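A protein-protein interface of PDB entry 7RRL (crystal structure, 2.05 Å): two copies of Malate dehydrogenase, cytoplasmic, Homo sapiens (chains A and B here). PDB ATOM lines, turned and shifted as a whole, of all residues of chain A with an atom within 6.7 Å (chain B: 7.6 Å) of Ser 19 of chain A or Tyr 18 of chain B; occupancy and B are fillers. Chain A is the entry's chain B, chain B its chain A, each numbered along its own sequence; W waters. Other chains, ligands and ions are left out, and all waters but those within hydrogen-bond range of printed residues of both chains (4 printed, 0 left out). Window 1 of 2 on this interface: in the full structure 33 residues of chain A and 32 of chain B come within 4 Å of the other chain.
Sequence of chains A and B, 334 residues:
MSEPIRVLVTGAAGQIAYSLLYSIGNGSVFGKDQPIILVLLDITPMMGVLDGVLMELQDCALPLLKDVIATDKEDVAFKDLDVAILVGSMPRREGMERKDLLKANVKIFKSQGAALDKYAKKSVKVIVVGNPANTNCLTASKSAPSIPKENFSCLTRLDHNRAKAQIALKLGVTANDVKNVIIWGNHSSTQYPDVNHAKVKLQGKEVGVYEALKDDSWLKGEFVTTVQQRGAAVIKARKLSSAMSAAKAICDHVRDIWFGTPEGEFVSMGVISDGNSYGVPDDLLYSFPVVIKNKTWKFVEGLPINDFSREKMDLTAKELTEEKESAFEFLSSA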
ATOM      1  N   GLY A  14       8.775 -17.862 -24.309  1.00  0.00           N
ATOM      2  CA  GLY A  14       8.967 -19.176 -24.893  1.00  0.00           C
ATOM      3  C   GLY A  14       8.139 -20.294 -24.236  1.00  0.00           C
ATOM      4  O   GLY A  14       7.392 -20.088 -23.278  1.00  0.00           O
ATOM      5  N   GLN A  15       8.339 -21.515 -24.764  1.00  0.00           N
ATOM      6  CA  GLN A  15       7.497 -22.666 -24.428  1.00  0.00           C
ATOM      7  C   GLN A  15       7.666 -23.109 -22.979  1.00  0.00           C
ATOM      8  O   GLN A  15       6.675 -23.380 -22.296  1.00  0.00           O
ATOM      9  CB  GLN A  15       7.814 -23.847 -25.352  1.00  0.00           C
ATOM     10  CG  GLN A  15       7.650 -23.549 -26.817  1.00  0.00           C
ATOM     11  CD  GLN A  15       6.363 -22.814 -27.108  1.00  0.00           C
ATOM     12  OE1 GLN A  15       5.267 -23.272 -26.746  1.00  0.00           O
ATOM     13  NE2 GLN A  15       6.484 -21.649 -27.747  1.00  0.00           N
ATOM     14  N   ILE A  16       8.915 -23.258 -22.516  1.00  0.00           N
ATOM     15  CA  ILE A  16       9.149 -23.691 -21.135  1.00  0.00           C
ATOM     16  C   ILE A  16       8.461 -22.744 -20.162  1.00  0.00           C
ATOM     17  O   ILE A  16       7.786 -23.178 -19.223  1.00  0.00           O
ATOM     18  CB  ILE A  16      10.658 -23.792 -20.828  1.00  0.00           C
ATOM     19  CG1 ILE A  16      11.319 -24.927 -21.614  1.00  0.00           C
ATOM     20  CG2 ILE A  16      10.873 -23.996 -19.311  1.00  0.00           C
ATOM     21  CD1 ILE A  16      12.856 -24.981 -21.445  1.00  0.00           C
ATOM     22  N   ALA A  17       8.670 -21.436 -20.344  1.00  0.00           N
ATOM     23  CA  ALA A  17       8.080 -20.461 -19.429  1.00  0.00           C
ATOM     24  C   ALA A  17       6.561 -20.528 -19.466  1.00  0.00           C
ATOM     25  O   ALA A  17       5.904 -20.417 -18.417  1.00  0.00           O
ATOM     26  CB  ALA A  17       8.554 -19.042 -19.757  1.00  0.00           C
ATOM     27  N   TYR A  18       5.986 -20.699 -20.659  1.00  0.00           N
ATOM     28  CA  TYR A  18       4.530 -20.809 -20.768  1.00  0.00           C
ATOM     29  C   TYR A  18       3.997 -21.926 -19.877  1.00  0.00           C
ATOM     30  O   TYR A  18       2.903 -21.807 -19.322  1.00  0.00           O
ATOM     31  CB  TYR A  18       4.107 -21.028 -22.238  1.00  0.00           C
ATOM     32  CG  TYR A  18       2.614 -20.816 -22.487  1.00  0.00           C
ATOM     33  CD1 TYR A  18       2.071 -19.535 -22.502  1.00  0.00           C
ATOM     34  CD2 TYR A  18       1.754 -21.900 -22.708  1.00  0.00           C
ATOM     35  CE1 TYR A  18       0.708 -19.329 -22.721  1.00  0.00           C
ATOM     36  CE2 TYR A  18       0.384 -21.705 -22.919  1.00  0.00           C
ATOM     37  CZ  TYR A  18      -0.129 -20.417 -22.931  1.00  0.00           C
ATOM     38  OH  TYR A  18      -1.478 -20.191 -23.147  1.00  0.00           O
ATOM     39  N   SER A  19       4.774 -22.993 -19.690  1.00  0.00           N
ATOM     40  CA  SER A  19       4.365 -24.085 -18.819  1.00  0.00           C
ATOM     41  C   SER A  19       4.727 -23.853 -17.359  1.00  0.00           C
ATOM     42  O   SER A  19       4.279 -24.619 -16.506  1.00  0.00           O
ATOM     43  CB  SER A  19       4.994 -25.403 -19.291  1.00  0.00           C
ATOM     44  OG  SER A  19       4.328 -25.906 -20.446  1.00  0.00           O
ATOM     45  N   LEU A  20       5.522 -22.828 -17.058  1.00  0.00           N
ATOM     46  CA  LEU A  20       6.081 -22.589 -15.732  1.00  0.00           C
ATOM     47  C   LEU A  20       5.347 -21.510 -14.931  1.00  0.00           C
ATOM     48  O   LEU A  20       5.143 -21.671 -13.720  1.00  0.00           O
ATOM     49  CB  LEU A  20       7.557 -22.206 -15.877  1.00  0.00           C
ATOM     50  CG  LEU A  20       8.307 -21.824 -14.620  1.00  0.00           C
ATOM     51  CD1 LEU A  20       8.336 -22.993 -13.652  1.00  0.00           C
ATOM     52  CD2 LEU A  20       9.716 -21.354 -14.963  1.00  0.00           C
ATOM     53  N   LEU A  21       4.930 -20.416 -15.572  1.00  0.00           N
ATOM     54  CA  LEU A  21       4.462 -19.240 -14.832  1.00  0.00           C
ATOM     55  C   LEU A  21       3.274 -19.549 -13.923  1.00  0.00           C
ATOM     56  O   LEU A  21       3.166 -18.980 -12.831  1.00  0.00           O
ATOM     57  CB  LEU A  21       4.110 -18.122 -15.813  1.00  0.00           C
ATOM     58  CG  LEU A  21       5.275 -17.759 -16.734  1.00  0.00           C
ATOM     59  CD1 LEU A  21       4.904 -16.576 -17.620  1.00  0.00           C
ATOM     60  CD2 LEU A  21       6.607 -17.491 -15.946  1.00  0.00           C
ATOM     61  N   TYR A  22       2.363 -20.432 -14.356  1.00  0.00           N
ATOM     62  CA  TYR A  22       1.200 -20.749 -13.529  1.00  0.00           C
ATOM     63  C   TYR A  22       1.617 -21.337 -12.187  1.00  0.00           C
ATOM     64  O   TYR A  22       1.102 -20.935 -11.136  1.00  0.00           O
ATOM     65  CB  TYR A  22       0.275 -21.722 -14.263  1.00  0.00           C
ATOM     66  CG  TYR A  22      -0.911 -22.193 -13.439  1.00  0.00           C
ATOM     67  CD1 TYR A  22      -1.727 -21.287 -12.766  1.00  0.00           C
ATOM     68  CD2 TYR A  22      -1.218 -23.543 -13.347  1.00  0.00           C
ATOM     69  CE1 TYR A  22      -2.817 -21.725 -12.008  1.00  0.00           C
ATOM     70  CE2 TYR A  22      -2.302 -23.987 -12.609  1.00  0.00           C
ATOM     71  CZ  TYR A  22      -3.098 -23.076 -11.938  1.00  0.00           C
ATOM     72  OH  TYR A  22      -4.175 -23.535 -11.206  1.00  0.00           O
ATOM     73  N   SER A  23       2.551 -22.302 -12.208  1.00  0.00           N
ATOM     74  CA  SER A  23       2.997 -22.943 -10.973  1.00  0.00           C
ATOM     75  C   SER A  23       3.641 -21.936 -10.016  1.00  0.00           C
ATOM     76  O   SER A  23       3.517 -22.068  -8.789  1.00  0.00           O
ATOM     77  CB  SER A  23       3.976 -24.072 -11.297  1.00  0.00           C
ATOM     78  OG  SER A  23       3.355 -25.128 -12.004  1.00  0.00           O
ATOM     79  N   VAL A 234      11.594 -37.174 -27.026  1.00  0.00           N
ATOM     80  CA  VAL A 234      10.371 -36.391 -26.875  1.00  0.00           C
ATOM     81  C   VAL A 234      10.229 -35.384 -28.016  1.00  0.00           C
ATOM     82  O   VAL A 234       9.135 -35.186 -28.551  1.00  0.00           O
ATOM     83  CB  VAL A 234      10.342 -35.691 -25.507  1.00  0.00           C
ATOM     84  CG1 VAL A 234       9.072 -34.864 -25.392  1.00  0.00           C
ATOM     85  CG2 VAL A 234      10.430 -36.709 -24.391  1.00  0.00           C
ATOM     86  N   ARG A 238       6.904 -35.120 -30.283  1.00  0.00           N
ATOM     87  CA  ARG A 238       6.043 -33.953 -30.212  1.00  0.00           C
ATOM     88  C   ARG A 238       6.374 -32.926 -31.275  1.00  0.00           C
ATOM     89  O   ARG A 238       5.529 -32.078 -31.566  1.00  0.00           O
ATOM     90  CB  ARG A 238       6.148 -33.325 -28.831  1.00  0.00           C
ATOM     91  CG  ARG A 238       5.267 -34.002 -27.831  1.00  0.00           C
ATOM     92  CD  ARG A 238       5.085 -33.117 -26.624  1.00  0.00           C
ATOM     93  NE  ARG A 238       4.133 -32.044 -26.869  1.00  0.00           N
ATOM     94  CZ  ARG A 238       4.439 -30.757 -26.771  1.00  0.00           C
ATOM     95  NH1 ARG A 238       5.676 -30.362 -26.519  1.00  0.00           N
ATOM     96  NH2 ARG A 238       3.483 -29.845 -26.929  1.00  0.00           N
ATOM     97  N   SER A 241       8.436 -28.488 -28.101  1.00  0.00           N
ATOM     98  CA  SER A 241       9.278 -28.449 -26.915  1.00  0.00           C
ATOM     99  C   SER A 241       9.045 -29.678 -26.038  1.00  0.00           C
ATOM    100  O   SER A 241       8.195 -30.537 -26.313  1.00  0.00           O
ATOM    101  CB  SER A 241       9.014 -27.166 -26.131  1.00  0.00           C
ATOM    102  N   SER A 242       9.850 -29.772 -24.987  1.00  0.00           N
ATOM    103  CA  SER A 242       9.616 -30.664 -23.859  1.00  0.00           C
ATOM    104  C   SER A 242       9.227 -29.857 -22.617  1.00  0.00           C
ATOM    105  O   SER A 242       9.640 -30.161 -21.491  1.00  0.00           O
ATOM    106  CB  SER A 242      10.852 -31.514 -23.595  1.00  0.00           C
ATOM    107  OG  SER A 242      10.599 -32.435 -22.563  1.00  0.00           O
ATOM    108  N   ALA A 243       8.388 -28.839 -22.825  1.00  0.00           N
ATOM    109  CA  ALA A 243       8.214 -27.767 -21.845  1.00  0.00           C
ATOM    110  C   ALA A 243       7.479 -28.220 -20.586  1.00  0.00           C
ATOM    111  O   ALA A 243       7.755 -27.710 -19.499  1.00  0.00           O
ATOM    112  CB  ALA A 243       7.469 -26.601 -22.491  1.00  0.00           C
ATOM    113  N   MET A 244       6.496 -29.117 -20.709  1.00  0.00           N
ATOM    114  CA  MET A 244       5.720 -29.518 -19.536  1.00  0.00           C
ATOM    115  C   MET A 244       6.608 -30.172 -18.470  1.00  0.00           C
ATOM    116  O   MET A 244       6.543 -29.815 -17.285  1.00  0.00           O
ATOM    117  CB  MET A 244       4.579 -30.461 -19.946  1.00  0.00           C
ATOM    118  CG  MET A 244       3.745 -30.926 -18.754  1.00  0.00           C
ATOM    119  SD  MET A 244       3.003 -32.560 -18.939  1.00  0.00           S
ATOM    120  CE  MET A 244       1.889 -32.272 -20.325  1.00  0.00           C
ATOM    121  N   SER A 245       7.441 -31.142 -18.864  1.00  0.00           N
ATOM    122  CA  SER A 245       8.261 -31.817 -17.863  1.00  0.00           C
ATOM    123  C   SER A 245       9.470 -30.978 -17.460  1.00  0.00           C
ATOM    124  O   SER A 245       9.934 -31.091 -16.318  1.00  0.00           O
ATOM    125  CB  SER A 245       8.724 -33.199 -18.356  1.00  0.00           C
ATOM    126  OG  SER A 245       9.240 -33.145 -19.674  1.00  0.00           O
ATOM    127  N   ALA A 246       9.985 -30.135 -18.359  1.00  0.00           N
ATOM    128  CA  ALA A 246      11.070 -29.227 -17.968  1.00  0.00           C
ATOM    129  C   ALA A 246      10.591 -28.219 -16.935  1.00  0.00           C
ATOM    130  O   ALA A 246      11.319 -27.898 -15.991  1.00  0.00           O
ATOM    131  CB  ALA A 246      11.653 -28.504 -19.191  1.00  0.00           C
ATOM    132  N   ALA A 247       9.368 -27.703 -17.100  1.00  0.00           N
ATOM    133  CA  ALA A 247       8.825 -26.748 -16.132  1.00  0.00           C
ATOM    134  C   ALA A 247       8.573 -27.409 -14.780  1.00  0.00           C
ATOM    135  O   ALA A 247       8.851 -26.820 -13.731  1.00  0.00           O
ATOM    136  CB  ALA A 247       7.526 -26.141 -16.671  1.00  0.00           C
ATOM    137  N   LYS A 248       7.998 -28.611 -14.781  1.00  0.00           N
ATOM    138  CA  LYS A 248       7.873 -29.366 -13.537  1.00  0.00           C
ATOM    139  C   LYS A 248       9.225 -29.525 -12.837  1.00  0.00           C
ATOM    140  O   LYS A 248       9.329 -29.359 -11.614  1.00  0.00           O
ATOM    141  CB  LYS A 248       7.255 -30.736 -13.826  1.00  0.00           C
ATOM    142  CG  LYS A 248       6.645 -31.371 -12.608  1.00  0.00           C
ATOM    143  CD  LYS A 248       7.589 -32.322 -11.912  1.00  0.00           C
ATOM    144  CE  LYS A 248       6.900 -32.871 -10.645  1.00  0.00           C
ATOM    145  NZ  LYS A 248       7.734 -33.946 -10.022  1.00  0.00           N
ATOM    146  N   CYS A 251      10.337 -26.324 -11.206  1.00  0.00           N
ATOM    147  CA  CYS A 251       9.585 -26.169  -9.963  1.00  0.00           C
ATOM    148  C   CYS A 251      10.159 -27.042  -8.849  1.00  0.00           C
ATOM    149  O   CYS A 251      10.309 -26.595  -7.708  1.00  0.00           O
ATOM    150  CB  CYS A 251       8.114 -26.525 -10.194  1.00  0.00           C
ATOM    151  SG  CYS A 251       7.211 -25.381 -11.214  1.00  0.00           S
ATOM    152  N   VAL B   9      -9.485 -36.831 -21.308  1.00  0.00           N
ATOM    153  CA  VAL B   9      -9.334 -35.528 -21.955  1.00  0.00           C
ATOM    154  C   VAL B   9      -9.281 -35.752 -23.465  1.00  0.00           C
ATOM    155  O   VAL B   9      -8.440 -36.518 -23.947  1.00  0.00           O
ATOM    156  CB  VAL B   9      -8.068 -34.793 -21.471  1.00  0.00           C
ATOM    157  CG1 VAL B   9      -7.908 -33.456 -22.197  1.00  0.00           C
ATOM    158  CG2 VAL B   9      -8.103 -34.597 -19.966  1.00  0.00           C
ATOM    159  N   GLY B  11      -9.146 -33.932 -27.499  1.00  0.00           N
ATOM    160  CA  GLY B  11      -8.203 -32.980 -28.060  1.00  0.00           C
ATOM    161  C   GLY B  11      -6.855 -33.032 -27.376  1.00  0.00           C
ATOM    162  O   GLY B  11      -6.203 -31.996 -27.188  1.00  0.00           O
ATOM    163  N   ALA B  12      -6.418 -34.231 -26.992  1.00  0.00           N
ATOM    164  CA  ALA B  12      -5.333 -34.330 -26.024  1.00  0.00           C
ATOM    165  C   ALA B  12      -3.963 -33.975 -26.593  1.00  0.00           C
ATOM    166  O   ALA B  12      -3.027 -33.790 -25.806  1.00  0.00           O
ATOM    167  CB  ALA B  12      -5.304 -35.732 -25.410  1.00  0.00           C
ATOM    168  N   ALA B  13      -3.808 -33.859 -27.913  1.00  0.00           N
ATOM    169  CA  ALA B  13      -2.533 -33.408 -28.457  1.00  0.00           C
ATOM    170  C   ALA B  13      -2.460 -31.895 -28.624  1.00  0.00           C
ATOM    171  O   ALA B  13      -1.450 -31.384 -29.112  1.00  0.00           O
ATOM    172  CB  ALA B  13      -2.249 -34.091 -29.798  1.00  0.00           C
ATOM    173  N   GLY B  14      -3.488 -31.162 -28.206  1.00  0.00           N
ATOM    174  CA  GLY B  14      -3.561 -29.743 -28.450  1.00  0.00           C
ATOM    175  C   GLY B  14      -3.080 -28.905 -27.280  1.00  0.00           C
ATOM    176  O   GLY B  14      -2.667 -29.394 -26.229  1.00  0.00           O
ATOM    177  N   GLN B  15      -3.194 -27.593 -27.478  1.00  0.00           N
ATOM    178  CA  GLN B  15      -2.517 -26.646 -26.594  1.00  0.00           C
ATOM    179  C   GLN B  15      -3.212 -26.531 -25.247  1.00  0.00           C
ATOM    180  O   GLN B  15      -2.549 -26.417 -24.214  1.00  0.00           O
ATOM    181  CB  GLN B  15      -2.426 -25.279 -27.276  1.00  0.00           C
ATOM    182  CG  GLN B  15      -1.203 -25.146 -28.176  1.00  0.00           C
ATOM    183  CD  GLN B  15       0.072 -25.405 -27.399  1.00  0.00           C
ATOM    184  OE1 GLN B  15       0.571 -26.539 -27.353  1.00  0.00           O
ATOM    185  NE2 GLN B  15       0.581 -24.360 -26.729  1.00  0.00           N
ATOM    186  N   ILE B  16      -4.549 -26.555 -25.232  1.00  0.00           N
ATOM    187  CA  ILE B  16      -5.256 -26.484 -23.955  1.00  0.00           C
ATOM    188  C   ILE B  16      -4.940 -27.712 -23.108  1.00  0.00           C
ATOM    189  O   ILE B  16      -4.646 -27.608 -21.911  1.00  0.00           O
ATOM    190  CB  ILE B  16      -6.768 -26.319 -24.180  1.00  0.00           C
ATOM    191  CG1 ILE B  16      -7.052 -24.902 -24.719  1.00  0.00           C
ATOM    192  CG2 ILE B  16      -7.506 -26.589 -22.874  1.00  0.00           C
ATOM    193  CD1 ILE B  16      -8.456 -24.691 -25.182  1.00  0.00           C
ATOM    194  N   ALA B  17      -4.973 -28.894 -23.721  1.00  0.00           N
ATOM    195  CA  ALA B  17      -4.679 -30.105 -22.963  1.00  0.00           C
ATOM    196  C   ALA B  17      -3.239 -30.107 -22.467  1.00  0.00           C
ATOM    197  O   ALA B  17      -2.957 -30.602 -21.369  1.00  0.00           O
ATOM    198  CB  ALA B  17      -4.972 -31.345 -23.826  1.00  0.00           C
ATOM    199  N   TYR B  18      -2.317 -29.549 -23.249  1.00  0.00           N
ATOM    200  CA  TYR B  18      -0.920 -29.507 -22.807  1.00  0.00           C
ATOM    201  C   TYR B  18      -0.749 -28.703 -21.514  1.00  0.00           C
ATOM    202  O   TYR B  18       0.097 -29.047 -20.679  1.00  0.00           O
ATOM    203  CB  TYR B  18      -0.036 -28.940 -23.916  1.00  0.00           C
ATOM    204  CG  TYR B  18       1.437 -29.217 -23.712  1.00  0.00           C
ATOM    205  CD1 TYR B  18       1.932 -30.514 -23.767  1.00  0.00           C
ATOM    206  CD2 TYR B  18       2.329 -28.181 -23.457  1.00  0.00           C
ATOM    207  CE1 TYR B  18       3.291 -30.777 -23.579  1.00  0.00           C
ATOM    208  CE2 TYR B  18       3.692 -28.431 -23.257  1.00  0.00           C
ATOM    209  CZ  TYR B  18       4.163 -29.730 -23.324  1.00  0.00           C
ATOM    210  OH  TYR B  18       5.507 -29.986 -23.143  1.00  0.00           O
ATOM    211  N   SER B  19      -1.544 -27.652 -21.314  1.00  0.00           N
ATOM    212  CA  SER B  19      -1.478 -26.885 -20.067  1.00  0.00           C
ATOM    213  C   SER B  19      -2.327 -27.478 -18.951  1.00  0.00           C
ATOM    214  O   SER B  19      -2.227 -27.006 -17.812  1.00  0.00           O
ATOM    215  CB  SER B  19      -1.925 -25.444 -20.303  1.00  0.00           C
ATOM    216  OG  SER B  19      -1.141 -24.832 -21.317  1.00  0.00           O
ATOM    217  N   LEU B  20      -3.168 -28.475 -19.253  1.00  0.00           N
ATOM    218  CA  LEU B  20      -4.108 -29.049 -18.288  1.00  0.00           C
ATOM    219  C   LEU B  20      -3.625 -30.357 -17.658  1.00  0.00           C
ATOM    220  O   LEU B  20      -3.894 -30.596 -16.474  1.00  0.00           O
ATOM    221  CB  LEU B  20      -5.481 -29.281 -18.959  1.00  0.00           C
ATOM    222  CG  LEU B  20      -6.610 -29.976 -18.184  1.00  0.00           C
ATOM    223  CD1 LEU B  20      -7.118 -29.084 -17.034  1.00  0.00           C
ATOM    224  CD2 LEU B  20      -7.795 -30.407 -19.084  1.00  0.00           C
ATOM    225  N   LEU B  21      -2.894 -31.195 -18.406  1.00  0.00           N
ATOM    226  CA  LEU B  21      -2.629 -32.563 -17.954  1.00  0.00           C
ATOM    227  C   LEU B  21      -1.809 -32.599 -16.671  1.00  0.00           C
ATOM    228  O   LEU B  21      -2.084 -33.413 -15.784  1.00  0.00           O
ATOM    229  CB  LEU B  21      -1.912 -33.350 -19.048  1.00  0.00           C
ATOM    230  CG  LEU B  21      -2.757 -33.563 -20.299  1.00  0.00           C
ATOM    231  CD1 LEU B  21      -2.065 -34.549 -21.243  1.00  0.00           C
ATOM    232  CD2 LEU B  21      -4.207 -34.008 -19.952  1.00  0.00           C
ATOM    233  N   TYR B  22      -0.794 -31.737 -16.557  1.00  0.00           N
ATOM    234  CA  TYR B  22       0.035 -31.749 -15.354  1.00  0.00           C
ATOM    235  C   TYR B  22      -0.797 -31.488 -14.096  1.00  0.00           C
ATOM    236  O   TYR B  22      -0.638 -32.182 -13.089  1.00  0.00           O
ATOM    237  CB  TYR B  22       1.171 -30.729 -15.480  1.00  0.00           C
ATOM    238  CG  TYR B  22       1.925 -30.498 -14.183  1.00  0.00           C
ATOM    239  CD1 TYR B  22       2.629 -31.528 -13.569  1.00  0.00           C
ATOM    240  CD2 TYR B  22       1.921 -29.258 -13.572  1.00  0.00           C
ATOM    241  CE1 TYR B  22       3.303 -31.335 -12.377  1.00  0.00           C
ATOM    242  CE2 TYR B  22       2.609 -29.045 -12.387  1.00  0.00           C
ATOM    243  CZ  TYR B  22       3.300 -30.090 -11.798  1.00  0.00           C
ATOM    244  OH  TYR B  22       3.967 -29.880 -10.619  1.00  0.00           O
ATOM    245  N   SER B  23      -1.702 -30.507 -14.141  1.00  0.00           N
ATOM    246  CA  SER B  23      -2.537 -30.218 -12.974  1.00  0.00           C
ATOM    247  C   SER B  23      -3.439 -31.389 -12.594  1.00  0.00           C
ATOM    248  O   SER B  23      -3.756 -31.575 -11.410  1.00  0.00           O
ATOM    249  CB  SER B  23      -3.389 -28.982 -13.228  1.00  0.00           C
ATOM    250  OG  SER B  23      -2.579 -27.825 -13.234  1.00  0.00           O
ATOM    251  N   VAL B  49       2.311 -37.179 -31.716  1.00  0.00           N
ATOM    252  CA  VAL B  49       2.445 -36.119 -30.723  1.00  0.00           C
ATOM    253  C   VAL B  49       2.042 -36.635 -29.352  1.00  0.00           C
ATOM    254  O   VAL B  49       2.697 -36.347 -28.339  1.00  0.00           O
ATOM    255  CB  VAL B  49       1.601 -34.898 -31.131  1.00  0.00           C
ATOM    256  CG1 VAL B  49       1.587 -33.859 -29.998  1.00  0.00           C
ATOM    257  CG2 VAL B  49       2.119 -34.316 -32.434  1.00  0.00           C
ATOM    258  N   GLY B  52       4.534 -38.452 -27.379  1.00  0.00           N
ATOM    259  CA  GLY B  52       5.441 -37.513 -26.735  1.00  0.00           C
ATOM    260  C   GLY B  52       4.871 -36.948 -25.450  1.00  0.00           C
ATOM    261  O   GLY B  52       5.592 -36.763 -24.473  1.00  0.00           O
ATOM    262  N   VAL B  53       3.559 -36.696 -25.428  1.00  0.00           N
ATOM    263  CA  VAL B  53       2.915 -36.202 -24.217  1.00  0.00           C
ATOM    264  C   VAL B  53       2.922 -37.269 -23.126  1.00  0.00           C
ATOM    265  O   VAL B  53       3.107 -36.965 -21.940  1.00  0.00           O
ATOM    266  CB  VAL B  53       1.490 -35.717 -24.542  1.00  0.00           C
ATOM    267  CG1 VAL B  53       0.790 -35.291 -23.277  1.00  0.00           C
ATOM    268  CG2 VAL B  53       1.554 -34.545 -25.518  1.00  0.00           C
ATOM    269  N   GLU B  56       6.378 -37.083 -21.579  1.00  0.00           N
ATOM    270  CA  GLU B  56       6.548 -35.968 -20.657  1.00  0.00           C
ATOM    271  C   GLU B  56       5.846 -36.224 -19.333  1.00  0.00           C
ATOM    272  O   GLU B  56       6.390 -35.903 -18.267  1.00  0.00           O
ATOM    273  CB  GLU B  56       6.029 -34.694 -21.301  1.00  0.00           C
ATOM    274  CG  GLU B  56       6.747 -34.361 -22.570  1.00  0.00           C
ATOM    275  CD  GLU B  56       6.801 -32.880 -22.776  1.00  0.00           C
ATOM    276  OE1 GLU B  56       7.388 -32.179 -21.911  1.00  0.00           O
ATOM    277  OE2 GLU B  56       6.247 -32.411 -23.792  1.00  0.00           O
ATOM    278  N   LEU B  57       4.639 -36.795 -19.377  1.00  0.00           N
ATOM    279  CA  LEU B  57       3.928 -37.118 -18.145  1.00  0.00           C
ATOM    280  C   LEU B  57       4.713 -38.121 -17.317  1.00  0.00           C
ATOM    281  O   LEU B  57       4.756 -38.032 -16.085  1.00  0.00           O
ATOM    282  CB  LEU B  57       2.537 -37.667 -18.463  1.00  0.00           C
ATOM    283  CG  LEU B  57       1.519 -36.633 -18.933  1.00  0.00           C
ATOM    284  CD1 LEU B  57       0.202 -37.327 -19.268  1.00  0.00           C
ATOM    285  CD2 LEU B  57       1.349 -35.570 -17.866  1.00  0.00           C
ATOM    286  N   ALA B 243      -4.434 -20.833 -23.695  1.00  0.00           N
ATOM    287  CA  ALA B 243      -4.309 -22.228 -23.287  1.00  0.00           C
ATOM    288  C   ALA B 243      -4.047 -22.333 -21.789  1.00  0.00           C
ATOM    289  O   ALA B 243      -4.743 -23.076 -21.087  1.00  0.00           O
ATOM    290  CB  ALA B 243      -3.216 -22.931 -24.084  1.00  0.00           C
ATOM    291  N   MET B 244      -3.061 -21.582 -21.288  1.00  0.00           N
ATOM    292  CA  MET B 244      -2.804 -21.562 -19.855  1.00  0.00           C
ATOM    293  C   MET B 244      -4.059 -21.181 -19.071  1.00  0.00           C
ATOM    294  O   MET B 244      -4.428 -21.854 -18.107  1.00  0.00           O
ATOM    295  CB  MET B 244      -1.660 -20.595 -19.526  1.00  0.00           C
ATOM    296  CG  MET B 244      -1.684 -20.162 -18.057  1.00  0.00           C
ATOM    297  SD  MET B 244      -0.666 -18.722 -17.647  1.00  0.00           S
ATOM    298  CE  MET B 244       0.754 -18.958 -18.710  1.00  0.00           C
ATOM    299  N   ALA B 247      -6.990 -23.732 -19.423  1.00  0.00           N
ATOM    300  CA  ALA B 247      -6.729 -24.913 -18.606  1.00  0.00           C
ATOM    301  C   ALA B 247      -6.919 -24.613 -17.131  1.00  0.00           C
ATOM    302  O   ALA B 247      -7.430 -25.447 -16.384  1.00  0.00           O
ATOM    303  CB  ALA B 247      -5.313 -25.436 -18.858  1.00  0.00           C
HETATM  304  O   HOH W   1       2.348 -27.493 -19.789  1.00  0.00           O
HETATM  305  O   HOH W   2       0.631 -23.559 -19.614  1.00  0.00           O
HETATM  306  O   HOH W   3       6.894 -29.404  -9.121  1.00  0.00           O
HETATM  307  O   HOH W   4       1.135 -31.668 -27.321  1.00  0.00           O
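Ser 19 of chain A touches one residue of chain B. Of chain A, only Ser 19 (3.8 Å), Arg 238 (3.4 Å), Ser 242 (3.8 Å), Ala 243 (3.1 Å) and Met 244 (2.8 Å) come within 4 Å of Tyr 18 of chain B. Printed residues of chain A within 4 Å of Ser 19 of chain B: Tyr 18 (3.8 Å). Ala 247 of chain A touches none of the printed residues of chain B. Ala 13 of chain B touches none of the printed residues of chain A. The nearest printed residue of chain A that does not touch Val 53 of chain B is Met 244 of chain A (4.4 Å).
Tyr 18 of chain A touches Ala 243 of chain B, and with the chains exchanged Ala 243 of chain A touches Tyr 18 of chain B. Tyr 18 of chain A touches Met 244 of chain B, and with the chains exchanged Met 244 of chain A touches Tyr 18 of chain B.
The side-chain hydroxyl (OH) of Tyr 18 of chain B is in hydrogen-bond range of the guanidinium group (NH1) of Arg 238 of chain A (3.4 Å). The backbone NH (N) of Ala 243 of chain A sits at hydrogen-bond distance from the side-chain hydroxyl (OH) of Tyr 18 of chain B (3.1 Å). N of Met 244 of chain A lies within hydrogen-bond range of OH of Tyr 18 of chain B, 2.8 Å away. OE2 of Glu 56 of chain B is in salt-bridge range of NH1 of Arg 238 of chain A. The side-chain carboxylate (OE1) of Glu 56 of chain B lies close to the side-chain hydroxyl (OG) of Ser 242 of chain A, 3.3 Å away. OE1 of Glu 56 of chain B lies within hydrogen-bond range of N of Met 244 of chain A, at 3.4 Å. OG of Ser 245 of chain A lies within hydrogen-bond range of OE1 of Glu 56 of chain B (3.1 Å). N of Ala 243 of chain B lies within hydrogen-bond range of OH of Tyr 18 of chain A (3.1 Å). The backbone NH (N) of Met 244 of chain B is in hydrogen-bond range of the side-chain hydroxyl (OH) of Tyr 18 of chain A.
The guanidinium group of Arg 238 of chain A sits at hydrogen-bond distance from the backbone carbonyl oxygen of Ser 241 of chain A, 2.5 Å away.
Water W1 bridges the side-chain hydroxyl of Ser 19 of chain A (2.6 Å) and the backbone carbonyl oxygen of Tyr 18 of chain B (2.9 Å). Water W2 bridges OG of Ser 19 of chain B and O of Tyr 18 of chain A.
Hydrophobic or aromatic side chains of chain B that line the printed part of chain A: Tyr 18, Tyr 22, Val 53, Leu 57, Ala 243 and Met 244.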
